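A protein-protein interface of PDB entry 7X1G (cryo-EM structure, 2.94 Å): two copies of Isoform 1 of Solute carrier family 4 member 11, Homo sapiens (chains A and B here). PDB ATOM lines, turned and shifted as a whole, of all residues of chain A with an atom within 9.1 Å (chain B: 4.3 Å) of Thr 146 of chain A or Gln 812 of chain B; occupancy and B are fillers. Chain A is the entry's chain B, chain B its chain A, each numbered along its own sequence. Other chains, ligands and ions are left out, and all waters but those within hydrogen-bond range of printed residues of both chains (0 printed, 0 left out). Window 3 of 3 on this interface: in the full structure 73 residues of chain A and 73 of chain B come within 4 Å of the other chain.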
ATOM      1  N   GLU A 143      -6.824 -13.208 -27.833  1.00  0.00           N
ATOM      2  CA  GLU A 143      -6.742 -14.330 -26.908  1.00  0.00           C
ATOM      3  C   GLU A 143      -6.863 -15.628 -27.698  1.00  0.00           C
ATOM      4  O   GLU A 143      -7.899 -15.887 -28.320  1.00  0.00           O
ATOM      5  CB  GLU A 143      -7.834 -14.235 -25.844  1.00  0.00           C
ATOM      6  CG  GLU A 143      -7.795 -15.348 -24.807  1.00  0.00           C
ATOM      7  CD  GLU A 143      -6.541 -15.307 -23.956  1.00  0.00           C
ATOM      8  OE1 GLU A 143      -5.957 -14.213 -23.807  1.00  0.00           O
ATOM      9  OE2 GLU A 143      -6.138 -16.370 -23.437  1.00  0.00           O
ATOM     10  N   THR A 144      -5.808 -16.440 -27.672  1.00  0.00           N
ATOM     11  CA  THR A 144      -5.755 -17.682 -28.429  1.00  0.00           C
ATOM     12  C   THR A 144      -6.229 -18.889 -27.631  1.00  0.00           C
ATOM     13  O   THR A 144      -6.198 -20.008 -28.152  1.00  0.00           O
ATOM     14  CB  THR A 144      -4.328 -17.935 -28.930  1.00  0.00           C
ATOM     15  OG1 THR A 144      -3.439 -18.043 -27.812  1.00  0.00           O
ATOM     16  CG2 THR A 144      -3.869 -16.801 -29.835  1.00  0.00           C
ATOM     17  N   ALA A 145      -6.664 -18.696 -26.390  1.00  0.00           N
ATOM     18  CA  ALA A 145      -7.134 -19.813 -25.583  1.00  0.00           C
ATOM     19  C   ALA A 145      -8.386 -20.425 -26.198  1.00  0.00           C
ATOM     20  O   ALA A 145      -9.250 -19.717 -26.723  1.00  0.00           O
ATOM     21  CB  ALA A 145      -7.418 -19.351 -24.156  1.00  0.00           C
ATOM     22  N   THR A 146      -8.481 -21.752 -26.130  1.00  0.00           N
ATOM     23  CA  THR A 146      -9.588 -22.472 -26.745  1.00  0.00           C
ATOM     24  C   THR A 146     -10.697 -22.815 -25.760  1.00  0.00           C
ATOM     25  O   THR A 146     -11.855 -22.956 -26.172  1.00  0.00           O
ATOM     26  CB  THR A 146      -9.084 -23.766 -27.393  1.00  0.00           C
ATOM     27  OG1 THR A 146      -8.511 -24.614 -26.392  1.00  0.00           O
ATOM     28  CG2 THR A 146      -8.041 -23.461 -28.458  1.00  0.00           C
ATOM     29  N   SER A 147     -10.378 -22.953 -24.479  1.00  0.00           N
ATOM     30  CA  SER A 147     -11.342 -23.349 -23.464  1.00  0.00           C
ATOM     31  C   SER A 147     -11.750 -22.150 -22.619  1.00  0.00           C
ATOM     32  O   SER A 147     -11.023 -21.158 -22.509  1.00  0.00           O
ATOM     33  CB  SER A 147     -10.770 -24.449 -22.565  1.00  0.00           C
ATOM     34  OG  SER A 147      -9.627 -23.991 -21.865  1.00  0.00           O
ATOM     35  N   LEU A 148     -12.936 -22.256 -22.017  1.00  0.00           N
ATOM     36  CA  LEU A 148     -13.429 -21.186 -21.156  1.00  0.00           C
ATOM     37  C   LEU A 148     -12.518 -20.988 -19.953  1.00  0.00           C
ATOM     38  O   LEU A 148     -12.259 -19.850 -19.541  1.00  0.00           O
ATOM     39  CB  LEU A 148     -14.851 -21.499 -20.696  1.00  0.00           C
ATOM     40  CG  LEU A 148     -15.967 -21.117 -21.665  1.00  0.00           C
ATOM     41  CD1 LEU A 148     -15.961 -22.042 -22.867  1.00  0.00           C
ATOM     42  CD2 LEU A 148     -17.315 -21.153 -20.964  1.00  0.00           C
ATOM     43  N   ASP A 149     -12.032 -22.084 -19.369  1.00  0.00           N
ATOM     44  CA  ASP A 149     -11.209 -21.974 -18.170  1.00  0.00           C
ATOM     45  C   ASP A 149      -9.952 -21.158 -18.437  1.00  0.00           C
ATOM     46  O   ASP A 149      -9.598 -20.279 -17.646  1.00  0.00           O
ATOM     47  CB  ASP A 149     -10.842 -23.367 -17.658  1.00  0.00           C
ATOM     48  CG  ASP A 149     -12.059 -24.199 -17.309  1.00  0.00           C
ATOM     49  OD1 ASP A 149     -13.181 -23.800 -17.686  1.00  0.00           O
ATOM     50  OD2 ASP A 149     -11.894 -25.252 -16.659  1.00  0.00           O
ATOM     51  N   ASN A 150      -9.268 -21.428 -19.550  1.00  0.00           N
ATOM     52  CA  ASN A 150      -8.047 -20.689 -19.860  1.00  0.00           C
ATOM     53  C   ASN A 150      -8.337 -19.215 -20.112  1.00  0.00           C
ATOM     54  O   ASN A 150      -7.602 -18.340 -19.636  1.00  0.00           O
ATOM     55  CB  ASN A 150      -7.355 -21.314 -21.071  1.00  0.00           C
ATOM     56  CG  ASN A 150      -6.977 -22.764 -20.842  1.00  0.00           C
ATOM     57  OD1 ASN A 150      -7.076 -23.274 -19.726  1.00  0.00           O
ATOM     58  ND2 ASN A 150      -6.544 -23.436 -21.900  1.00  0.00           N
ATOM     59  N   VAL A 151      -9.402 -18.917 -20.859  1.00  0.00           N
ATOM     60  CA  VAL A 151      -9.737 -17.526 -21.153  1.00  0.00           C
ATOM     61  C   VAL A 151     -10.027 -16.771 -19.863  1.00  0.00           C
ATOM     62  O   VAL A 151      -9.528 -15.661 -19.645  1.00  0.00           O
ATOM     63  CB  VAL A 151     -10.930 -17.453 -22.123  1.00  0.00           C
ATOM     64  CG1 VAL A 151     -11.363 -16.008 -22.317  1.00  0.00           C
ATOM     65  CG2 VAL A 151     -10.580 -18.088 -23.459  1.00  0.00           C
ATOM     66  N   LEU A 152     -10.839 -17.366 -18.987  1.00  0.00           N
ATOM     67  CA  LEU A 152     -11.188 -16.694 -17.743  1.00  0.00           C
ATOM     68  C   LEU A 152      -9.988 -16.580 -16.811  1.00  0.00           C
ATOM     69  O   LEU A 152      -9.856 -15.578 -16.100  1.00  0.00           O
ATOM     70  CB  LEU A 152     -12.335 -17.429 -17.055  1.00  0.00           C
ATOM     71  CG  LEU A 152     -13.646 -17.466 -17.846  1.00  0.00           C
ATOM     72  CD1 LEU A 152     -14.708 -18.220 -17.075  1.00  0.00           C
ATOM     73  CD2 LEU A 152     -14.126 -16.061 -18.179  1.00  0.00           C
ATOM     74  N   THR A 154      -6.853 -16.189 -17.799  1.00  0.00           N
ATOM     75  CA  THR A 154      -6.075 -15.075 -18.331  1.00  0.00           C
ATOM     76  C   THR A 154      -6.726 -13.740 -17.986  1.00  0.00           C
ATOM     77  O   THR A 154      -6.042 -12.789 -17.590  1.00  0.00           O
ATOM     78  CB  THR A 154      -5.918 -15.217 -19.845  1.00  0.00           C
ATOM     79  OG1 THR A 154      -5.257 -16.452 -20.148  1.00  0.00           O
ATOM     80  CG2 THR A 154      -5.109 -14.059 -20.413  1.00  0.00           C
ATOM     81  N   LEU A 234     -11.444 -12.349 -28.610  1.00  0.00           N
ATOM     82  CA  LEU A 234     -10.857 -13.609 -29.035  1.00  0.00           C
ATOM     83  C   LEU A 234     -10.408 -13.527 -30.488  1.00  0.00           C
ATOM     84  O   LEU A 234     -11.014 -12.836 -31.311  1.00  0.00           O
ATOM     85  CB  LEU A 234     -11.859 -14.753 -28.863  1.00  0.00           C
ATOM     86  CG  LEU A 234     -12.627 -14.768 -27.538  1.00  0.00           C
ATOM     87  CD1 LEU A 234     -13.701 -15.839 -27.553  1.00  0.00           C
ATOM     88  CD2 LEU A 234     -11.680 -14.974 -26.368  1.00  0.00           C
ATOM     89  N   VAL A 235      -9.326 -14.245 -30.797  1.00  0.00           N
ATOM     90  CA  VAL A 235      -8.817 -14.269 -32.165  1.00  0.00           C
ATOM     91  C   VAL A 235      -9.855 -14.871 -33.103  1.00  0.00           C
ATOM     92  O   VAL A 235     -10.065 -14.381 -34.220  1.00  0.00           O
ATOM     93  CB  VAL A 235      -7.486 -15.041 -32.229  1.00  0.00           C
ATOM     94  CG1 VAL A 235      -7.029 -15.197 -33.673  1.00  0.00           C
ATOM     95  CG2 VAL A 235      -6.424 -14.335 -31.405  1.00  0.00           C
ATOM     96  N   ARG A 236     -10.518 -15.937 -32.669  1.00  0.00           N
ATOM     97  CA  ARG A 236     -11.517 -16.627 -33.464  1.00  0.00           C
ATOM     98  C   ARG A 236     -12.810 -16.744 -32.673  1.00  0.00           C
ATOM     99  O   ARG A 236     -12.786 -16.764 -31.438  1.00  0.00           O
ATOM    100  CB  ARG A 236     -11.035 -18.030 -33.858  1.00  0.00           C
ATOM    101  CG  ARG A 236     -10.151 -18.059 -35.099  1.00  0.00           C
ATOM    102  CD  ARG A 236      -9.422 -19.389 -35.262  1.00  0.00           C
ATOM    103  NE  ARG A 236      -8.873 -19.890 -34.006  1.00  0.00           N
ATOM    104  CZ  ARG A 236      -7.595 -19.829 -33.654  1.00  0.00           C
ATOM    105  NH1 ARG A 236      -6.683 -19.272 -34.437  1.00  0.00           N
ATOM    106  NH2 ARG A 236      -7.220 -20.335 -32.483  1.00  0.00           N
ATOM    107  N   PRO A 237     -13.958 -16.829 -33.372  1.00  0.00           N
ATOM    108  CA  PRO A 237     -15.181 -17.036 -32.601  1.00  0.00           C
ATOM    109  C   PRO A 237     -15.191 -18.406 -31.952  1.00  0.00           C
ATOM    110  O   PRO A 237     -14.815 -19.361 -32.624  1.00  0.00           O
ATOM    111  CB  PRO A 237     -16.285 -16.914 -33.645  1.00  0.00           C
ATOM    112  CG  PRO A 237     -15.637 -17.152 -34.954  1.00  0.00           C
ATOM    113  CD  PRO A 237     -14.245 -16.638 -34.808  1.00  0.00           C
ATOM    114  N   GLN A 238     -15.550 -18.497 -30.674  1.00  0.00           N
ATOM    115  CA  GLN A 238     -15.546 -19.726 -29.929  1.00  0.00           C
ATOM    116  C   GLN A 238     -16.894 -20.002 -29.372  1.00  0.00           C
ATOM    117  O   GLN A 238     -17.523 -19.113 -28.865  1.00  0.00           O
ATOM    118  CB  GLN A 238     -14.596 -19.558 -28.772  1.00  0.00           C
ATOM    119  CG  GLN A 238     -13.204 -19.202 -29.213  1.00  0.00           C
ATOM    120  CD  GLN A 238     -12.237 -19.141 -28.073  1.00  0.00           C
ATOM    121  OE1 GLN A 238     -12.551 -19.540 -26.958  1.00  0.00           O
ATOM    122  NE2 GLN A 238     -11.046 -18.635 -28.346  1.00  0.00           N
ATOM    123  N   ASN A 239     -17.373 -21.236 -29.405  1.00  0.00           N
ATOM    124  CA  ASN A 239     -18.645 -21.629 -28.804  1.00  0.00           C
ATOM    125  C   ASN A 239     -18.437 -21.411 -27.351  1.00  0.00           C
ATOM    126  O   ASN A 239     -17.367 -21.604 -26.880  1.00  0.00           O
ATOM    127  CB  ASN A 239     -18.852 -23.098 -29.084  1.00  0.00           C
ATOM    128  CG  ASN A 239     -20.265 -23.558 -28.975  1.00  0.00           C
ATOM    129  OD1 ASN A 239     -20.908 -23.853 -29.965  1.00  0.00           O
ATOM    130  ND2 ASN A 239     -20.722 -23.720 -27.774  1.00  0.00           N
ATOM    131  N   TRP A 240     -19.415 -20.953 -26.607  1.00  0.00           N
ATOM    132  CA  TRP A 240     -19.184 -20.645 -25.224  1.00  0.00           C
ATOM    133  C   TRP A 240     -20.477 -20.975 -24.589  1.00  0.00           C
ATOM    134  O   TRP A 240     -20.709 -20.629 -23.450  1.00  0.00           O
ATOM    135  CB  TRP A 240     -18.884 -19.171 -25.029  1.00  0.00           C
ATOM    136  CG  TRP A 240     -17.463 -18.825 -24.794  1.00  0.00           C
ATOM    137  CD1 TRP A 240     -16.424 -19.021 -25.636  1.00  0.00           C
ATOM    138  CD2 TRP A 240     -16.927 -18.184 -23.647  1.00  0.00           C
ATOM    139  NE1 TRP A 240     -15.263 -18.574 -25.080  1.00  0.00           N
ATOM    140  CE2 TRP A 240     -15.548 -18.050 -23.852  1.00  0.00           C
ATOM    141  CE3 TRP A 240     -17.477 -17.725 -22.454  1.00  0.00           C
ATOM    142  CZ2 TRP A 240     -14.715 -17.477 -22.916  1.00  0.00           C
ATOM    143  CZ3 TRP A 240     -16.648 -17.167 -21.530  1.00  0.00           C
ATOM    144  CH2 TRP A 240     -15.282 -17.041 -21.761  1.00  0.00           C
ATOM    145  N   CYS A 245     -22.563 -19.574 -29.558  1.00  0.00           N
ATOM    146  CA  CYS A 245     -21.752 -20.419 -30.424  1.00  0.00           C
ATOM    147  C   CYS A 245     -20.666 -19.658 -31.174  1.00  0.00           C
ATOM    148  O   CYS A 245     -19.736 -20.292 -31.684  1.00  0.00           O
ATOM    149  CB  CYS A 245     -22.651 -21.139 -31.431  1.00  0.00           C
ATOM    150  SG  CYS A 245     -23.929 -22.167 -30.675  1.00  0.00           S
ATOM    151  N   PRO A 598     -21.444 -25.624 -39.010  1.00  0.00           N
ATOM    152  CA  PRO A 598     -20.910 -24.694 -38.005  1.00  0.00           C
ATOM    153  C   PRO A 598     -19.541 -25.070 -37.465  1.00  0.00           C
ATOM    154  O   PRO A 598     -18.976 -24.296 -36.681  1.00  0.00           O
ATOM    155  CB  PRO A 598     -21.966 -24.744 -36.895  1.00  0.00           C
ATOM    156  CG  PRO A 598     -22.543 -26.109 -36.993  1.00  0.00           C
ATOM    157  CD  PRO A 598     -22.468 -26.519 -38.442  1.00  0.00           C
ATOM    158  N   TYR A 599     -18.989 -26.219 -37.855  1.00  0.00           N
ATOM    159  CA  TYR A 599     -17.717 -26.679 -37.315  1.00  0.00           C
ATOM    160  C   TYR A 599     -16.536 -26.406 -38.234  1.00  0.00           C
ATOM    161  O   TYR A 599     -15.394 -26.403 -37.759  1.00  0.00           O
ATOM    162  CB  TYR A 599     -17.784 -28.182 -37.023  1.00  0.00           C
ATOM    163  CG  TYR A 599     -18.679 -28.529 -35.857  1.00  0.00           C
ATOM    164  CD1 TYR A 599     -18.299 -28.234 -34.556  1.00  0.00           C
ATOM    165  CD2 TYR A 599     -19.904 -29.150 -36.056  1.00  0.00           C
ATOM    166  CE1 TYR A 599     -19.114 -28.547 -33.488  1.00  0.00           C
ATOM    167  CE2 TYR A 599     -20.724 -29.467 -34.992  1.00  0.00           C
ATOM    168  CZ  TYR A 599     -20.324 -29.164 -33.710  1.00  0.00           C
ATOM    169  OH  TYR A 599     -21.135 -29.476 -32.644  1.00  0.00           O
ATOM    170  N   LEU A 600     -16.773 -26.181 -39.522  1.00  0.00           N
ATOM    171  CA  LEU A 600     -15.691 -25.882 -40.444  1.00  0.00           C
ATOM    172  C   LEU A 600     -15.159 -24.472 -40.204  1.00  0.00           C
ATOM    173  O   LEU A 600     -15.858 -23.594 -39.692  1.00  0.00           O
ATOM    174  CB  LEU A 600     -16.163 -26.021 -41.891  1.00  0.00           C
ATOM    175  CG  LEU A 600     -16.427 -27.438 -42.408  1.00  0.00           C
ATOM    176  CD1 LEU A 600     -16.842 -27.394 -43.869  1.00  0.00           C
ATOM    177  CD2 LEU A 600     -15.206 -28.326 -42.233  1.00  0.00           C
ATOM    178  N   HIS A 601     -13.902 -24.265 -40.584  1.00  0.00           N
ATOM    179  CA  HIS A 601     -13.306 -22.946 -40.467  1.00  0.00           C
ATOM    180  C   HIS A 601     -14.061 -21.958 -41.356  1.00  0.00           C
ATOM    181  O   HIS A 601     -14.532 -22.322 -42.436  1.00  0.00           O
ATOM    182  CB  HIS A 601     -11.837 -22.981 -40.874  1.00  0.00           C
ATOM    183  CG  HIS A 601     -10.956 -23.707 -39.907  1.00  0.00           C
ATOM    184  ND1 HIS A 601     -10.596 -23.179 -38.686  1.00  0.00           N
ATOM    185  CD2 HIS A 601     -10.356 -24.919 -39.984  1.00  0.00           C
ATOM    186  CE1 HIS A 601      -9.814 -24.036 -38.052  1.00  0.00           C
ATOM    187  NE2 HIS A 601      -9.654 -25.100 -38.817  1.00  0.00           N
ATOM    188  N   PRO A 602     -14.194 -20.698 -40.926  1.00  0.00           N
ATOM    189  CA  PRO A 602     -14.907 -19.729 -41.777  1.00  0.00           C
ATOM    190  C   PRO A 602     -14.326 -19.632 -43.176  1.00  0.00           C
ATOM    191  O   PRO A 602     -15.080 -19.565 -44.155  1.00  0.00           O
ATOM    192  CB  PRO A 602     -14.764 -18.412 -41.004  1.00  0.00           C
ATOM    193  CG  PRO A 602     -14.527 -18.818 -39.594  1.00  0.00           C
ATOM    194  CD  PRO A 602     -13.748 -20.094 -39.659  1.00  0.00           C
ATOM    195  N   LEU B 807     -11.502 -33.608 -37.503  1.00  0.00           N
ATOM    196  CA  LEU B 807     -11.260 -32.404 -36.716  1.00  0.00           C
ATOM    197  C   LEU B 807     -10.161 -31.546 -37.327  1.00  0.00           C
ATOM    198  O   LEU B 807     -10.128 -30.331 -37.105  1.00  0.00           O
ATOM    199  CB  LEU B 807     -10.898 -32.783 -35.279  1.00  0.00           C
ATOM    200  CG  LEU B 807     -10.560 -31.629 -34.331  1.00  0.00           C
ATOM    201  CD1 LEU B 807     -11.771 -30.737 -34.119  1.00  0.00           C
ATOM    202  CD2 LEU B 807     -10.049 -32.165 -33.005  1.00  0.00           C
ATOM    203  N   LYS B 810     -12.021 -29.324 -39.271  1.00  0.00           N
ATOM    204  CA  LYS B 810     -13.033 -28.631 -38.491  1.00  0.00           C
ATOM    205  C   LYS B 810     -12.378 -27.583 -37.593  1.00  0.00           C
ATOM    206  O   LYS B 810     -11.164 -27.366 -37.622  1.00  0.00           O
ATOM    207  CB  LYS B 810     -13.843 -29.628 -37.662  1.00  0.00           C
ATOM    208  CG  LYS B 810     -14.429 -30.789 -38.456  1.00  0.00           C
ATOM    209  CD  LYS B 810     -15.840 -30.487 -38.929  1.00  0.00           C
ATOM    210  CE  LYS B 810     -16.485 -31.702 -39.574  1.00  0.00           C
ATOM    211  NZ  LYS B 810     -16.694 -32.809 -38.599  1.00  0.00           N
ATOM    212  N   GLU B 811     -13.198 -26.923 -36.778  1.00  0.00           N
ATOM    213  CA  GLU B 811     -12.741 -25.905 -35.839  1.00  0.00           C
ATOM    214  C   GLU B 811     -12.908 -26.440 -34.422  1.00  0.00           C
ATOM    215  O   GLU B 811     -14.013 -26.821 -34.026  1.00  0.00           O
ATOM    216  CB  GLU B 811     -13.524 -24.605 -36.021  1.00  0.00           C
ATOM    217  CG  GLU B 811     -13.013 -23.443 -35.183  1.00  0.00           C
ATOM    218  CD  GLU B 811     -11.696 -22.892 -35.688  1.00  0.00           C
ATOM    219  OE1 GLU B 811     -11.713 -22.092 -36.648  1.00  0.00           O
ATOM    220  OE2 GLU B 811     -10.642 -23.258 -35.128  1.00  0.00           O
ATOM    221  N   GLN B 812     -11.809 -26.465 -33.665  1.00  0.00           N
ATOM    222  CA  GLN B 812     -11.868 -26.970 -32.298  1.00  0.00           C
ATOM    223  C   GLN B 812     -12.752 -26.089 -31.424  1.00  0.00           C
ATOM    224  O   GLN B 812     -13.524 -26.593 -30.600  1.00  0.00           O
ATOM    225  CB  GLN B 812     -10.458 -27.062 -31.713  1.00  0.00           C
ATOM    226  CG  GLN B 812     -10.401 -27.627 -30.301  1.00  0.00           C
ATOM    227  CD  GLN B 812      -9.034 -27.475 -29.666  1.00  0.00           C
ATOM    228  OE1 GLN B 812      -8.276 -26.566 -30.004  1.00  0.00           O
ATOM    229  NE2 GLN B 812      -8.711 -28.369 -28.739  1.00  0.00           N
ATOM    230  N   THR B 813     -12.653 -24.770 -31.587  1.00  0.00           N
ATOM    231  CA  THR B 813     -13.399 -23.843 -30.747  1.00  0.00           C
ATOM    232  C   THR B 813     -14.893 -23.844 -31.039  1.00  0.00           C
ATOM    233  O   THR B 813     -15.653 -23.240 -30.275  1.00  0.00           O
ATOM    234  CB  THR B 813     -12.850 -22.426 -30.917  1.00  0.00           C
ATOM    235  OG1 THR B 813     -12.862 -22.067 -32.304  1.00  0.00           O
ATOM    236  CG2 THR B 813     -11.429 -22.335 -30.384  1.00  0.00           C
ATOM    237  N   ALA B 814     -15.333 -24.496 -32.113  1.00  0.00           N
ATOM    238  CA  ALA B 814     -16.747 -24.547 -32.456  1.00  0.00           C
ATOM    239  C   ALA B 814     -17.499 -25.649 -31.723  1.00  0.00           C
ATOM    240  O   ALA B 814     -18.726 -25.727 -31.848  1.00  0.00           O
ATOM    241  CB  ALA B 814     -16.915 -24.738 -33.966  1.00  0.00           C
ATOM    242  N   TYR B 815     -16.804 -26.498 -30.973  1.00  0.00           N
ATOM    243  CA  TYR B 815     -17.446 -27.580 -30.249  1.00  0.00           C
ATOM    244  C   TYR B 815     -18.040 -27.071 -28.939  1.00  0.00           C
ATOM    245  O   TYR B 815     -17.696 -25.983 -28.471  1.00  0.00           O
ATOM    246  CB  TYR B 815     -16.443 -28.695 -29.978  1.00  0.00           C
ATOM    247  CG  TYR B 815     -16.196 -29.583 -31.175  1.00  0.00           C
ATOM    248  CD1 TYR B 815     -15.239 -29.253 -32.124  1.00  0.00           C
ATOM    249  CD2 TYR B 815     -16.927 -30.749 -31.362  1.00  0.00           C
ATOM    250  CE1 TYR B 815     -15.012 -30.060 -33.221  1.00  0.00           C
ATOM    251  CE2 TYR B 815     -16.708 -31.562 -32.456  1.00  0.00           C
ATOM    252  CZ  TYR B 815     -15.748 -31.213 -33.382  1.00  0.00           C
ATOM    253  OH  TYR B 815     -15.525 -32.020 -34.474  1.00  0.00           O
ATOM    254  N   ILE B 821     -13.178 -32.526 -26.768  1.00  0.00           N
ATOM    255  CA  ILE B 821     -12.254 -32.012 -27.773  1.00  0.00           C
ATOM    256  C   ILE B 821     -11.678 -30.709 -27.271  1.00  0.00           C
ATOM    257  O   ILE B 821     -10.471 -30.520 -27.279  1.00  0.00           O
ATOM    258  CB  ILE B 821     -12.923 -31.855 -29.166  1.00  0.00           C
ATOM    259  CG1 ILE B 821     -13.080 -33.232 -29.824  1.00  0.00           C
ATOM    260  CG2 ILE B 821     -12.119 -30.930 -30.068  1.00  0.00           C
ATOM    261  CD1 ILE B 821     -14.098 -33.303 -30.942  1.00  0.00           C
ATOM    262  N   ARG B 822     -12.536 -29.799 -26.839  1.00  0.00           N
ATOM    263  CA  ARG B 822     -12.073 -28.527 -26.288  1.00  0.00           C
ATOM    264  C   ARG B 822     -11.301 -28.680 -24.984  1.00  0.00           C
ATOM    265  O   ARG B 822     -10.339 -27.955 -24.753  1.00  0.00           O
ATOM    266  CB  ARG B 822     -13.217 -27.531 -26.171  1.00  0.00           C
ATOM    267  CG  ARG B 822     -13.603 -26.996 -27.536  1.00  0.00           C
ATOM    268  CD  ARG B 822     -14.700 -25.970 -27.463  1.00  0.00           C
ATOM    269  NE  ARG B 822     -14.254 -24.661 -26.983  1.00  0.00           N
ATOM    270  CZ  ARG B 822     -15.069 -23.676 -26.608  1.00  0.00           C
ATOM    271  NH1 ARG B 822     -16.384 -23.843 -26.630  1.00  0.00           N
ATOM    272  NH2 ARG B 822     -14.575 -22.511 -26.189  1.00  0.00           N
ATOM    273  N   VAL B 824      -9.318 -31.207 -23.947  1.00  0.00           N
ATOM    274  CA  VAL B 824      -7.968 -31.755 -24.116  1.00  0.00           C
ATOM    275  C   VAL B 824      -7.186 -30.851 -25.085  1.00  0.00           C
ATOM    276  O   VAL B 824      -7.751 -30.414 -26.081  1.00  0.00           O
ATOM    277  CB  VAL B 824      -8.007 -33.222 -24.616  1.00  0.00           C
ATOM    278  CG1 VAL B 824      -6.602 -33.789 -24.776  1.00  0.00           C
ATOM    279  CG2 VAL B 824      -8.797 -34.106 -23.653  1.00  0.00           C
ATOM    280  N   GLN B 826      -5.221 -29.565 -28.190  1.00  0.00           N
ATOM    281  CA  GLN B 826      -5.271 -30.088 -29.550  1.00  0.00           C
ATOM    282  C   GLN B 826      -4.025 -30.884 -29.907  1.00  0.00           C
ATOM    283  O   GLN B 826      -4.100 -31.782 -30.751  1.00  0.00           O
ATOM    284  CB  GLN B 826      -5.460 -28.944 -30.548  1.00  0.00           C
ATOM    285  CG  GLN B 826      -5.859 -29.403 -31.941  1.00  0.00           C
ATOM    286  CD  GLN B 826      -6.153 -28.247 -32.877  1.00  0.00           C
ATOM    287  OE1 GLN B 826      -5.988 -27.083 -32.514  1.00  0.00           O
ATOM    288  NE2 GLN B 826      -6.595 -28.564 -34.088  1.00  0.00           N
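The side-chain carboxylate (OE1) of Glu 811 of chain B lies within hydrogen-bond range of a ring nitrogen (ND1) of His 601 of chain A (2.6 Å).
A ring nitrogen (NE2) of His 601 of chain A sits at hydrogen-bond distance from the backbone carbonyl oxygen (O) of Lys 810 of chain B, at 3.0 Å.
NH2 of Arg 822 of chain B lies within hydrogen-bond range of O of Thr 146 of chain A (2.8 Å).
The backbone NH (N) of Glu 811 of chain B is in hydrogen-bond range of the backbone carbonyl oxygen (O) of Tyr 599 of chain A (2.5 Å).
The side-chain carboxylate (OE2) of Glu 811 of chain B lies within salt-bridge range of the guanidinium group (NE) of Arg 236 of chain A (3.97 Å).
The backbone carbonyl oxygen (O) of Ala 814 of chain B lies close to the side-chain amide oxygen (OD1) of Asn 239 of chain A (3.4 Å).
The guanidinium group of Arg 822 of chain B sits at hydrogen-bond distance from the backbone carbonyl oxygen of Asn 239 of chain A, 2.5 Å away.
O of Thr 813 of chain B sits at hydrogen-bond distance from N of Asn 239 of chain A.
The side-chain hydroxyl of Thr 813 of chain B is in hydrogen-bond range of the backbone carbonyl oxygen of Pro 237 of chain A (3.4 Å).
N of Asn 239 of chain A sits close to O of Cys 245 of chain A (3.4 Å).
O of Ala 145 of chain A sits at hydrogen-bond distance from NE2 of Gln 238 of chain A, at 2.7 Å.
The backbone carbonyl oxygen (O) of Ile 821 of chain B lies within hydrogen-bond range of the side-chain amide nitrogen (NE2) of Gln 812 of chain B.
NE1 of Trp 240 of chain A is in hydrogen-bond range of OE1 of Gln 238 of chain A.
The backbone carbonyl oxygen (O) of Tyr 815 of chain B lies within hydrogen-bond range of the guanidinium group (NH1) of Arg 822 of chain B (3.1 Å).
The backbone carbonyl oxygen of Val 824 of chain B lies within hydrogen-bond range of the side-chain amide nitrogen of Gln 812 of chain B (3.5 Å).
Thr 146 of chain A touches Gln 812 of chain B (CG2 to OE1, 3.5 Å).
NH2 of Arg 822 of chain B touches CD1 of Leu 148 of chain A, 3.6 Å away.
Gln 238 of chain A touches Thr 813 of chain B (CA to O, 3.5 Å).
NH2 of Arg 822 of chain B touches OE1 of Gln 238 of chain A, 3.7 Å away.
Asn 239 of chain A touches Tyr 815 of chain B (CB to O, 3.2 Å).
NH2 of Arg 822 of chain B touches CD1 of Trp 240 of chain A, at 3.99 Å.
Tyr 599 of chain A touches Lys 810 of chain B.
Ala 814 of chain B touches Tyr 599 of chain A.
Tyr 599 of chain A touches Tyr 815 of chain B.
Leu 600 of chain A touches Lys 810 of chain B (CD2 to CD, 3.999 Å).
Of chain B, only Gln 812 and Arg 822 come within 4 Å of Thr 146 of chain A.
Gln 812 of chain B touches just one residue of chain A: Thr 146.
Thr 813 of chain B touches three residues of chain A.
Printed residues of chain B within 4 Å of Tyr 599 of chain A: Lys 810, Glu 811, Ala 814 and Tyr 815.
Of the printed residues of chain B, His 601 of chain A touches Lys 810 (3.0 Å) and Glu 811 (2.6 Å).
Printed residues of chain B within 4 Å of Leu 600 of chain A: Lys 810 (3.999 Å).
Printed residues of chain B within 4 Å of Trp 240 of chain A: Arg 822 (3.99 Å).
Of the printed residues of chain A, Glu 811 of chain B touches Arg 236 (3.8 Å), Tyr 599 (2.5 Å) and His 601 (2.6 Å).
Gln 826 of chain B touches none of the printed residues of chain A.
The nearest printed residue of chain B that does not touch Asn 239 of chain A is Gln 812 of chain B (6.5 Å).
Printed residues of chain A that touch a printed residue of chain B: Thr 146, Leu 148, Arg 236, Pro 237, Gln 238, Asn 239, Trp 240, Pro 598, Tyr 599, Leu 600 and His 601.
Hydrophobic or aromatic side chains of chain A that line the printed part of chain B: Leu 148, Trp 240, Tyr 599, Leu 600 and His 601.
Among the printed residues, Asp or Glu carboxylates within 4 Å of a Lys or Arg side-chain nitrogen of the other chain: Arg 236 of chain A with Glu 811 of chain B.
No position is printed for both chains.
Of the 20 pairs that touch across the chains among the printed residues, none has its exchanged pair printed and touching as well.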
